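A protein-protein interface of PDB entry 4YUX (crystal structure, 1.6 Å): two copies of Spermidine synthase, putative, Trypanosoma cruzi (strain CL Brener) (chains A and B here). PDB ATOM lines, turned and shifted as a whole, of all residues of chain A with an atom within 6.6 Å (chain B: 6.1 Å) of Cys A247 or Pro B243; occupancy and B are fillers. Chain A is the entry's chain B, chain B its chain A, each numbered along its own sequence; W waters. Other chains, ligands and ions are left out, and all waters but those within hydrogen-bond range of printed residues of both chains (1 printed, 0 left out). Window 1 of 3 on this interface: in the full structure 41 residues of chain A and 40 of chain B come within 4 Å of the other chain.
NE2 of Gln A30 sits close to NE1 of Trp B61, at 2.9 Å.
OE1 of Gln A30 is in hydrogen-bond range of SG of Cys A247, 3.4 Å away.
The side-chain hydroxyl (OG1) of Thr B244 lies within hydrogen-bond range of the side-chain carboxylate (OD2) of Asp B77, 2.7 Å away.
OG of Ser A212 lies within hydrogen-bond range of N of Trp A214 (3.0 Å).
Among the printed residues, pairs that only touch across the chains: Trp A214 with Asp B77 (3.9 Å), Trp A214 with Val B80 (3.5 Å), Trp A214 with His B241 (3.6 Å), Trp A214 with Pro B243 (3.4 Å), Pro A243 with Cys B247 (3.3 Å), Cys A247 with Trp B61 (3.7 Å), Cys A247 with Pro B243 (3.3 Å) and Ser A249 with His B241 (3.5 Å).
Cys A247 touches just these residues of chain B: Trp B61 (3.7 Å) and Pro B243 (3.3 Å).
Of the printed residues of chain B, Trp A214 touches Asp B77, Val B80, His B241 and Pro B243.
Of the printed residues of chain A, Trp B61 touches Gln A30 and Cys A247.
Trp A27 touches none of the printed residues of chain B.
Leu A215 touches none of the printed residues of chain B.
The nearest printed residue of chain A that does not touch Cys B247 is Gly A248 (4.4 Å).
Of the 12 printed residues of chain A, 5 touch a printed residue of chain B.
Hydrophobic or aromatic side chains of chain A that line the printed part of chain B: Trp A214 and Pro A243.
Of the 13 printed residues of chain B, 6 touch a printed residue of chain A.
Printed residues of chain B that touch a printed residue of chain A: Trp B61, Asp B77, Val B80, His B241, Pro B243 and Cys B247.
Among the printed residues, 9 pairs touch across the chains.
Among the printed residues, no Asp or Glu carboxylate lies within 4 Å of a Lys or Arg side-chain nitrogen of the other chain.
Pro A243 touches Cys B247, and with the chains exchanged Cys A247 touches Pro B243.
7 positions are printed for both chains.
Of the 9 pairs that touch across the chains among the printed residues, 2 have their exchanged pair printed and touching as well.
Water W1 lies within hydrogen-bond range of O of Cys A247, O of Gly B248 and NE1 of Trp A214.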
ATOM      1  N   TRP A  27      18.078 -27.830   5.395  1.00  0.00           N
ATOM      2  CA  TRP A  27      17.204 -26.609   5.161  1.00  0.00           C
ATOM      3  C   TRP A  27      18.119 -25.493   4.726  1.00  0.00           C
ATOM      4  O   TRP A  27      18.455 -24.594   5.485  1.00  0.00           O
ATOM      5  CB  TRP A  27      16.361 -26.287   6.425  1.00  0.00           C
ATOM      6  CG  TRP A  27      17.033 -26.445   7.733  1.00  0.00           C
ATOM      7  CD1 TRP A  27      17.882 -25.590   8.358  1.00  0.00           C
ATOM      8  CD2 TRP A  27      16.937 -27.601   8.566  1.00  0.00           C
ATOM      9  NE1 TRP A  27      18.244 -26.090   9.608  1.00  0.00           N
ATOM     10  CE2 TRP A  27      17.714 -27.364   9.704  1.00  0.00           C
ATOM     11  CE3 TRP A  27      16.253 -28.799   8.422  1.00  0.00           C
ATOM     12  CZ2 TRP A  27      17.832 -28.290  10.775  1.00  0.00           C
ATOM     13  CZ3 TRP A  27      16.347 -29.759   9.499  1.00  0.00           C
ATOM     14  CH2 TRP A  27      17.160 -29.474  10.643  1.00  0.00           C
ATOM     15  N   GLN A  30      18.516 -21.058   5.501  1.00  0.00           N
ATOM     16  CA  GLN A  30      17.800 -20.629   6.684  1.00  0.00           C
ATOM     17  C   GLN A  30      18.392 -21.178   7.954  1.00  0.00           C
ATOM     18  O   GLN A  30      18.978 -22.280   7.926  1.00  0.00           O
ATOM     19  CB  GLN A  30      16.316 -21.009   6.622  1.00  0.00           C
ATOM     20  CG  GLN A  30      16.049 -22.547   6.841  1.00  0.00           C
ATOM     21  CD  GLN A  30      14.609 -22.836   6.566  1.00  0.00           C
ATOM     22  OE1 GLN A  30      13.826 -23.063   7.545  1.00  0.00           O
ATOM     23  NE2 GLN A  30      14.218 -22.898   5.340  1.00  0.00           N
ATOM     24  N   SER A 212       8.506 -31.460   7.972  1.00  0.00           N
ATOM     25  CA  SER A 212       7.918 -30.147   7.600  1.00  0.00           C
ATOM     26  C   SER A 212       7.259 -30.126   6.240  1.00  0.00           C
ATOM     27  O   SER A 212       7.912 -30.388   5.213  1.00  0.00           O
ATOM     28  CB  SER A 212       9.033 -29.114   7.595  1.00  0.00           C
ATOM     29  OG  SER A 212       8.568 -27.851   7.062  1.00  0.00           O
ATOM     30  N   TRP A 214       6.833 -27.487   4.664  1.00  0.00           N
ATOM     31  CA  TRP A 214       7.486 -26.382   3.888  1.00  0.00           C
ATOM     32  C   TRP A 214       8.774 -26.848   3.267  1.00  0.00           C
ATOM     33  O   TRP A 214       9.280 -26.214   2.320  1.00  0.00           O
ATOM     34  CB  TRP A 214       7.825 -25.241   4.893  1.00  0.00           C
ATOM     35  CG  TRP A 214       6.551 -24.642   5.468  1.00  0.00           C
ATOM     36  CD1 TRP A 214       6.038 -24.821   6.738  1.00  0.00           C
ATOM     37  CD2 TRP A 214       5.652 -23.780   4.788  1.00  0.00           C
ATOM     38  NE1 TRP A 214       4.846 -24.130   6.879  1.00  0.00           N
ATOM     39  CE2 TRP A 214       4.611 -23.457   5.706  1.00  0.00           C
ATOM     40  CE3 TRP A 214       5.691 -23.148   3.526  1.00  0.00           C
ATOM     41  CZ2 TRP A 214       3.540 -22.543   5.348  1.00  0.00           C
ATOM     42  CZ3 TRP A 214       4.648 -22.262   3.193  1.00  0.00           C
ATOM     43  CH2 TRP A 214       3.602 -22.002   4.113  1.00  0.00           C
ATOM     44  N   LEU A 215       9.346 -27.907   3.838  1.00  0.00           N
ATOM     45  CA  LEU A 215      10.748 -28.308   3.459  1.00  0.00           C
ATOM     46  C   LEU A 215      10.809 -29.706   2.872  1.00  0.00           C
ATOM     47  O   LEU A 215      11.647 -29.993   1.957  1.00  0.00           O
ATOM     48  CB  LEU A 215      11.734 -28.216   4.679  1.00  0.00           C
ATOM     49  CG  LEU A 215      11.861 -26.823   5.367  1.00  0.00           C
ATOM     50  CD1 LEU A 215      12.542 -26.995   6.722  1.00  0.00           C
ATOM     51  CD2 LEU A 215      12.627 -25.874   4.456  1.00  0.00           C
ATOM     52  N   VAL A 242       5.099 -26.052  16.373  1.00  0.00           N
ATOM     53  CA  VAL A 242       6.301 -26.172  17.202  1.00  0.00           C
ATOM     54  C   VAL A 242       7.376 -25.167  16.769  1.00  0.00           C
ATOM     55  O   VAL A 242       8.069 -25.311  15.709  1.00  0.00           O
ATOM     56  CB  VAL A 242       6.852 -27.583  17.053  1.00  0.00           C
ATOM     57  CG1 VAL A 242       8.198 -27.775  17.767  1.00  0.00           C
ATOM     58  CG2 VAL A 242       5.843 -28.654  17.543  1.00  0.00           C
ATOM     59  N   PRO A 243       7.546 -24.151  17.592  1.00  0.00           N
ATOM     60  CA  PRO A 243       8.397 -23.042  17.131  1.00  0.00           C
ATOM     61  C   PRO A 243       9.865 -23.464  16.836  1.00  0.00           C
ATOM     62  O   PRO A 243      10.545 -22.799  16.047  1.00  0.00           O
ATOM     63  CB  PRO A 243       8.407 -22.100  18.360  1.00  0.00           C
ATOM     64  CG  PRO A 243       6.969 -22.222  18.901  1.00  0.00           C
ATOM     65  CD  PRO A 243       6.682 -23.773  18.724  1.00  0.00           C
ATOM     66  N   TYR A 245      11.036 -26.353  15.691  1.00  0.00           N
ATOM     67  CA  TYR A 245      11.330 -27.181  14.569  1.00  0.00           C
ATOM     68  C   TYR A 245      11.421 -26.318  13.299  1.00  0.00           C
ATOM     69  O   TYR A 245      10.659 -25.397  13.205  1.00  0.00           O
ATOM     70  CB  TYR A 245      10.259 -28.303  14.421  1.00  0.00           C
ATOM     71  CG  TYR A 245      10.594 -29.349  13.357  1.00  0.00           C
ATOM     72  CD1 TYR A 245      11.552 -30.389  13.626  1.00  0.00           C
ATOM     73  CD2 TYR A 245      10.039 -29.306  12.045  1.00  0.00           C
ATOM     74  CE1 TYR A 245      11.899 -31.335  12.675  1.00  0.00           C
ATOM     75  CE2 TYR A 245      10.376 -30.270  11.104  1.00  0.00           C
ATOM     76  CZ  TYR A 245      11.308 -31.289  11.422  1.00  0.00           C
ATOM     77  OH  TYR A 245      11.635 -32.246  10.448  1.00  0.00           O
ATOM     78  N   PRO A 246      12.312 -26.643  12.318  1.00  0.00           N
ATOM     79  CA  PRO A 246      12.485 -25.651  11.240  1.00  0.00           C
ATOM     80  C   PRO A 246      11.168 -25.320  10.525  1.00  0.00           C
ATOM     81  O   PRO A 246      10.421 -26.212  10.105  1.00  0.00           O
ATOM     82  CB  PRO A 246      13.496 -26.300  10.327  1.00  0.00           C
ATOM     83  CG  PRO A 246      14.387 -27.097  11.359  1.00  0.00           C
ATOM     84  CD  PRO A 246      13.361 -27.702  12.327  1.00  0.00           C
ATOM     85  N   CYS A 247      10.954 -24.006  10.326  1.00  0.00           N
ATOM     86  CA  CYS A 247       9.764 -23.379   9.730  1.00  0.00           C
ATOM     87  C   CYS A 247       8.550 -23.367  10.677  1.00  0.00           C
ATOM     88  O   CYS A 247       7.513 -22.779  10.313  1.00  0.00           O
ATOM     89  CB  CYS A 247       9.325 -24.007   8.388  1.00  0.00           C
ATOM     90  SG  CYS A 247      10.550 -23.787   7.073  1.00  0.00           S
ATOM     91  N   GLY A 248       8.693 -23.952  11.896  1.00  0.00           N
ATOM     92  CA  GLY A 248       7.635 -23.721  12.912  1.00  0.00           C
ATOM     93  C   GLY A 248       6.512 -24.701  12.986  1.00  0.00           C
ATOM     94  O   GLY A 248       5.530 -24.480  13.809  1.00  0.00           O
ATOM     95  N   SER A 249       6.486 -25.621  12.052  1.00  0.00           N
ATOM     96  CA  SER A 249       5.469 -26.681  12.155  1.00  0.00           C
ATOM     97  C   SER A 249       6.030 -28.013  11.858  1.00  0.00           C
ATOM     98  O   SER A 249       7.006 -28.150  11.085  1.00  0.00           O
ATOM     99  CB  SER A 249       4.333 -26.465  11.299  1.00  0.00           C
ATOM    100  OG  SER A 249       4.710 -26.568   9.997  1.00  0.00           O
ATOM    101  N   MET B  32      15.301 -15.680  13.878  1.00  0.00           N
ATOM    102  CA  MET B  32      15.242 -16.326  12.622  1.00  0.00           C
ATOM    103  C   MET B  32      16.272 -15.664  11.654  1.00  0.00           C
ATOM    104  O   MET B  32      16.486 -14.377  11.720  1.00  0.00           O
ATOM    105  CB  MET B  32      13.799 -16.289  12.068  1.00  0.00           C
ATOM    106  CG  MET B  32      13.748 -16.943  10.640  1.00  0.00           C
ATOM    107  SD  MET B  32      14.268 -18.654  10.807  1.00  0.00           S
ATOM    108  CE  MET B  32      13.757 -19.211   9.194  1.00  0.00           C
ATOM    109  N   TRP B  61      13.092 -19.428  -0.314  1.00  0.00           N
ATOM    110  CA  TRP B  61      12.370 -18.205   0.137  1.00  0.00           C
ATOM    111  C   TRP B  61      12.231 -17.104  -0.871  1.00  0.00           C
ATOM    112  O   TRP B  61      11.278 -16.325  -0.742  1.00  0.00           O
ATOM    113  CB  TRP B  61      13.077 -17.650   1.403  1.00  0.00           C
ATOM    114  CG  TRP B  61      13.070 -18.764   2.446  1.00  0.00           C
ATOM    115  CD1 TRP B  61      14.094 -19.684   2.753  1.00  0.00           C
ATOM    116  CD2 TRP B  61      11.928 -19.214   3.179  1.00  0.00           C
ATOM    117  NE1 TRP B  61      13.631 -20.625   3.708  1.00  0.00           N
ATOM    118  CE2 TRP B  61      12.289 -20.379   3.900  1.00  0.00           C
ATOM    119  CE3 TRP B  61      10.589 -18.771   3.246  1.00  0.00           C
ATOM    120  CZ2 TRP B  61      11.377 -21.098   4.706  1.00  0.00           C
ATOM    121  CZ3 TRP B  61       9.702 -19.474   4.105  1.00  0.00           C
ATOM    122  CH2 TRP B  61      10.080 -20.641   4.765  1.00  0.00           C
ATOM    123  N   ASP B  77       6.271 -17.826   1.262  1.00  0.00           N
ATOM    124  CA  ASP B  77       5.169 -18.062   2.225  1.00  0.00           C
ATOM    125  C   ASP B  77       4.214 -16.877   2.319  1.00  0.00           C
ATOM    126  O   ASP B  77       3.329 -16.891   3.176  1.00  0.00           O
ATOM    127  CB  ASP B  77       5.678 -18.490   3.637  1.00  0.00           C
ATOM    128  CG  ASP B  77       6.416 -17.382   4.343  1.00  0.00           C
ATOM    129  OD1 ASP B  77       6.502 -16.260   3.743  1.00  0.00           O
ATOM    130  OD2 ASP B  77       6.878 -17.613   5.480  1.00  0.00           O
ATOM    131  N   VAL B  80       0.136 -17.235   2.812  1.00  0.00           N
ATOM    132  CA  VAL B  80      -0.629 -17.719   3.975  1.00  0.00           C
ATOM    133  C   VAL B  80      -1.413 -16.579   4.678  1.00  0.00           C
ATOM    134  O   VAL B  80      -2.645 -16.631   4.763  1.00  0.00           O
ATOM    135  CB  VAL B  80       0.290 -18.355   5.075  1.00  0.00           C
ATOM    136  CG1 VAL B  80      -0.626 -18.826   6.255  1.00  0.00           C
ATOM    137  CG2 VAL B  80       1.051 -19.578   4.486  1.00  0.00           C
ATOM    138  N   HIS B 241      -0.147 -20.834  10.071  1.00  0.00           N
ATOM    139  CA  HIS B 241       1.283 -21.307  10.007  1.00  0.00           C
ATOM    140  C   HIS B 241       2.062 -20.401   9.050  1.00  0.00           C
ATOM    141  O   HIS B 241       1.938 -20.506   7.827  1.00  0.00           O
ATOM    142  CB  HIS B 241       1.312 -22.729   9.472  1.00  0.00           C
ATOM    143  CG  HIS B 241       0.744 -23.752  10.395  1.00  0.00           C
ATOM    144  ND1 HIS B 241      -0.559 -24.224  10.384  1.00  0.00           N
ATOM    145  CD2 HIS B 241       1.392 -24.492  11.318  1.00  0.00           C
ATOM    146  CE1 HIS B 241      -0.705 -25.180  11.307  1.00  0.00           C
ATOM    147  NE2 HIS B 241       0.453 -25.340  11.885  1.00  0.00           N
ATOM    148  N   VAL B 242       2.924 -19.540   9.609  1.00  0.00           N
ATOM    149  CA  VAL B 242       3.741 -18.622   8.806  1.00  0.00           C
ATOM    150  C   VAL B 242       5.179 -18.775   9.259  1.00  0.00           C
ATOM    151  O   VAL B 242       5.590 -18.282  10.314  1.00  0.00           O
ATOM    152  CB  VAL B 242       3.262 -17.164   8.941  1.00  0.00           C
ATOM    153  CG1 VAL B 242       4.217 -16.256   8.151  1.00  0.00           C
ATOM    154  CG2 VAL B 242       1.821 -16.971   8.467  1.00  0.00           C
ATOM    155  N   PRO B 243       5.981 -19.472   8.424  1.00  0.00           N
ATOM    156  CA  PRO B 243       7.401 -19.769   8.871  1.00  0.00           C
ATOM    157  C   PRO B 243       8.209 -18.497   9.216  1.00  0.00           C
ATOM    158  O   PRO B 243       9.100 -18.512  10.112  1.00  0.00           O
ATOM    159  CB  PRO B 243       7.992 -20.401   7.636  1.00  0.00           C
ATOM    160  CG  PRO B 243       6.843 -21.210   7.032  1.00  0.00           C
ATOM    161  CD  PRO B 243       5.599 -20.249   7.225  1.00  0.00           C
ATOM    162  N   THR B 244       7.907 -17.422   8.450  1.00  0.00           N
ATOM    163  CA  THR B 244       8.705 -16.206   8.621  1.00  0.00           C
ATOM    164  C   THR B 244       8.135 -15.106   9.492  1.00  0.00           C
ATOM    165  O   THR B 244       8.508 -13.906   9.342  1.00  0.00           O
ATOM    166  CB  THR B 244       9.201 -15.654   7.250  1.00  0.00           C
ATOM    167  OG1 THR B 244       8.076 -15.366   6.460  1.00  0.00           O
ATOM    168  CG2 THR B 244      10.048 -16.765   6.607  1.00  0.00           C
ATOM    169  N   TYR B 245       7.273 -15.481  10.423  1.00  0.00           N
ATOM    170  CA  TYR B 245       6.976 -14.671  11.534  1.00  0.00           C
ATOM    171  C   TYR B 245       7.548 -15.328  12.765  1.00  0.00           C
ATOM    172  O   TYR B 245       7.546 -16.537  12.887  1.00  0.00           O
ATOM    173  CB  TYR B 245       5.423 -14.427  11.626  1.00  0.00           C
ATOM    174  CG  TYR B 245       5.004 -13.413  12.690  1.00  0.00           C
ATOM    175  CD1 TYR B 245       5.038 -12.000  12.421  1.00  0.00           C
ATOM    176  CD2 TYR B 245       4.592 -13.834  13.973  1.00  0.00           C
ATOM    177  CE1 TYR B 245       4.666 -11.082  13.368  1.00  0.00           C
ATOM    178  CE2 TYR B 245       4.255 -12.894  14.939  1.00  0.00           C
ATOM    179  CZ  TYR B 245       4.295 -11.521  14.617  1.00  0.00           C
ATOM    180  OH  TYR B 245       3.954 -10.574  15.569  1.00  0.00           O
ATOM    181  N   PRO B 246       7.990 -14.518  13.725  1.00  0.00           N
ATOM    182  CA  PRO B 246       8.637 -15.137  14.863  1.00  0.00           C
ATOM    183  C   PRO B 246       7.852 -16.244  15.570  1.00  0.00           C
ATOM    184  O   PRO B 246       6.680 -16.030  15.905  1.00  0.00           O
ATOM    185  CB  PRO B 246       8.932 -13.941  15.814  1.00  0.00           C
ATOM    186  CG  PRO B 246       9.093 -12.812  14.846  1.00  0.00           C
ATOM    187  CD  PRO B 246       8.120 -13.052  13.702  1.00  0.00           C
ATOM    188  N   CYS B 247       8.550 -17.383  15.761  1.00  0.00           N
ATOM    189  CA  CYS B 247       8.051 -18.671  16.349  1.00  0.00           C
ATOM    190  C   CYS B 247       7.183 -19.436  15.408  1.00  0.00           C
ATOM    191  O   CYS B 247       6.696 -20.520  15.793  1.00  0.00           O
ATOM    192  CB  CYS B 247       7.252 -18.488  17.687  1.00  0.00           C
ATOM    193  SG  CYS B 247       8.303 -17.819  19.013  1.00  0.00           S
ATOM    194  N   GLY B 248       6.883 -18.857  14.223  1.00  0.00           N
ATOM    195  CA  GLY B 248       6.286 -19.749  13.156  1.00  0.00           C
ATOM    196  C   GLY B 248       4.790 -19.652  13.048  1.00  0.00           C
ATOM    197  O   GLY B 248       4.169 -20.423  12.282  1.00  0.00           O
ATOM    198  N   SER B 249       4.197 -18.890  13.882  1.00  0.00           N
ATOM    199  CA  SER B 249       2.719 -18.725  13.777  1.00  0.00           C
ATOM    200  C   SER B 249       2.294 -17.329  14.116  1.00  0.00           C
ATOM    201  O   SER B 249       3.079 -16.559  14.715  1.00  0.00           O
ATOM    202  CB  SER B 249       2.045 -19.638  14.637  1.00  0.00           C
ATOM    203  OG  SER B 249       2.242 -19.377  15.974  1.00  0.00           O
HETATM  204  O   HOH W   1       4.941 -22.612   9.973  1.00  0.00           O
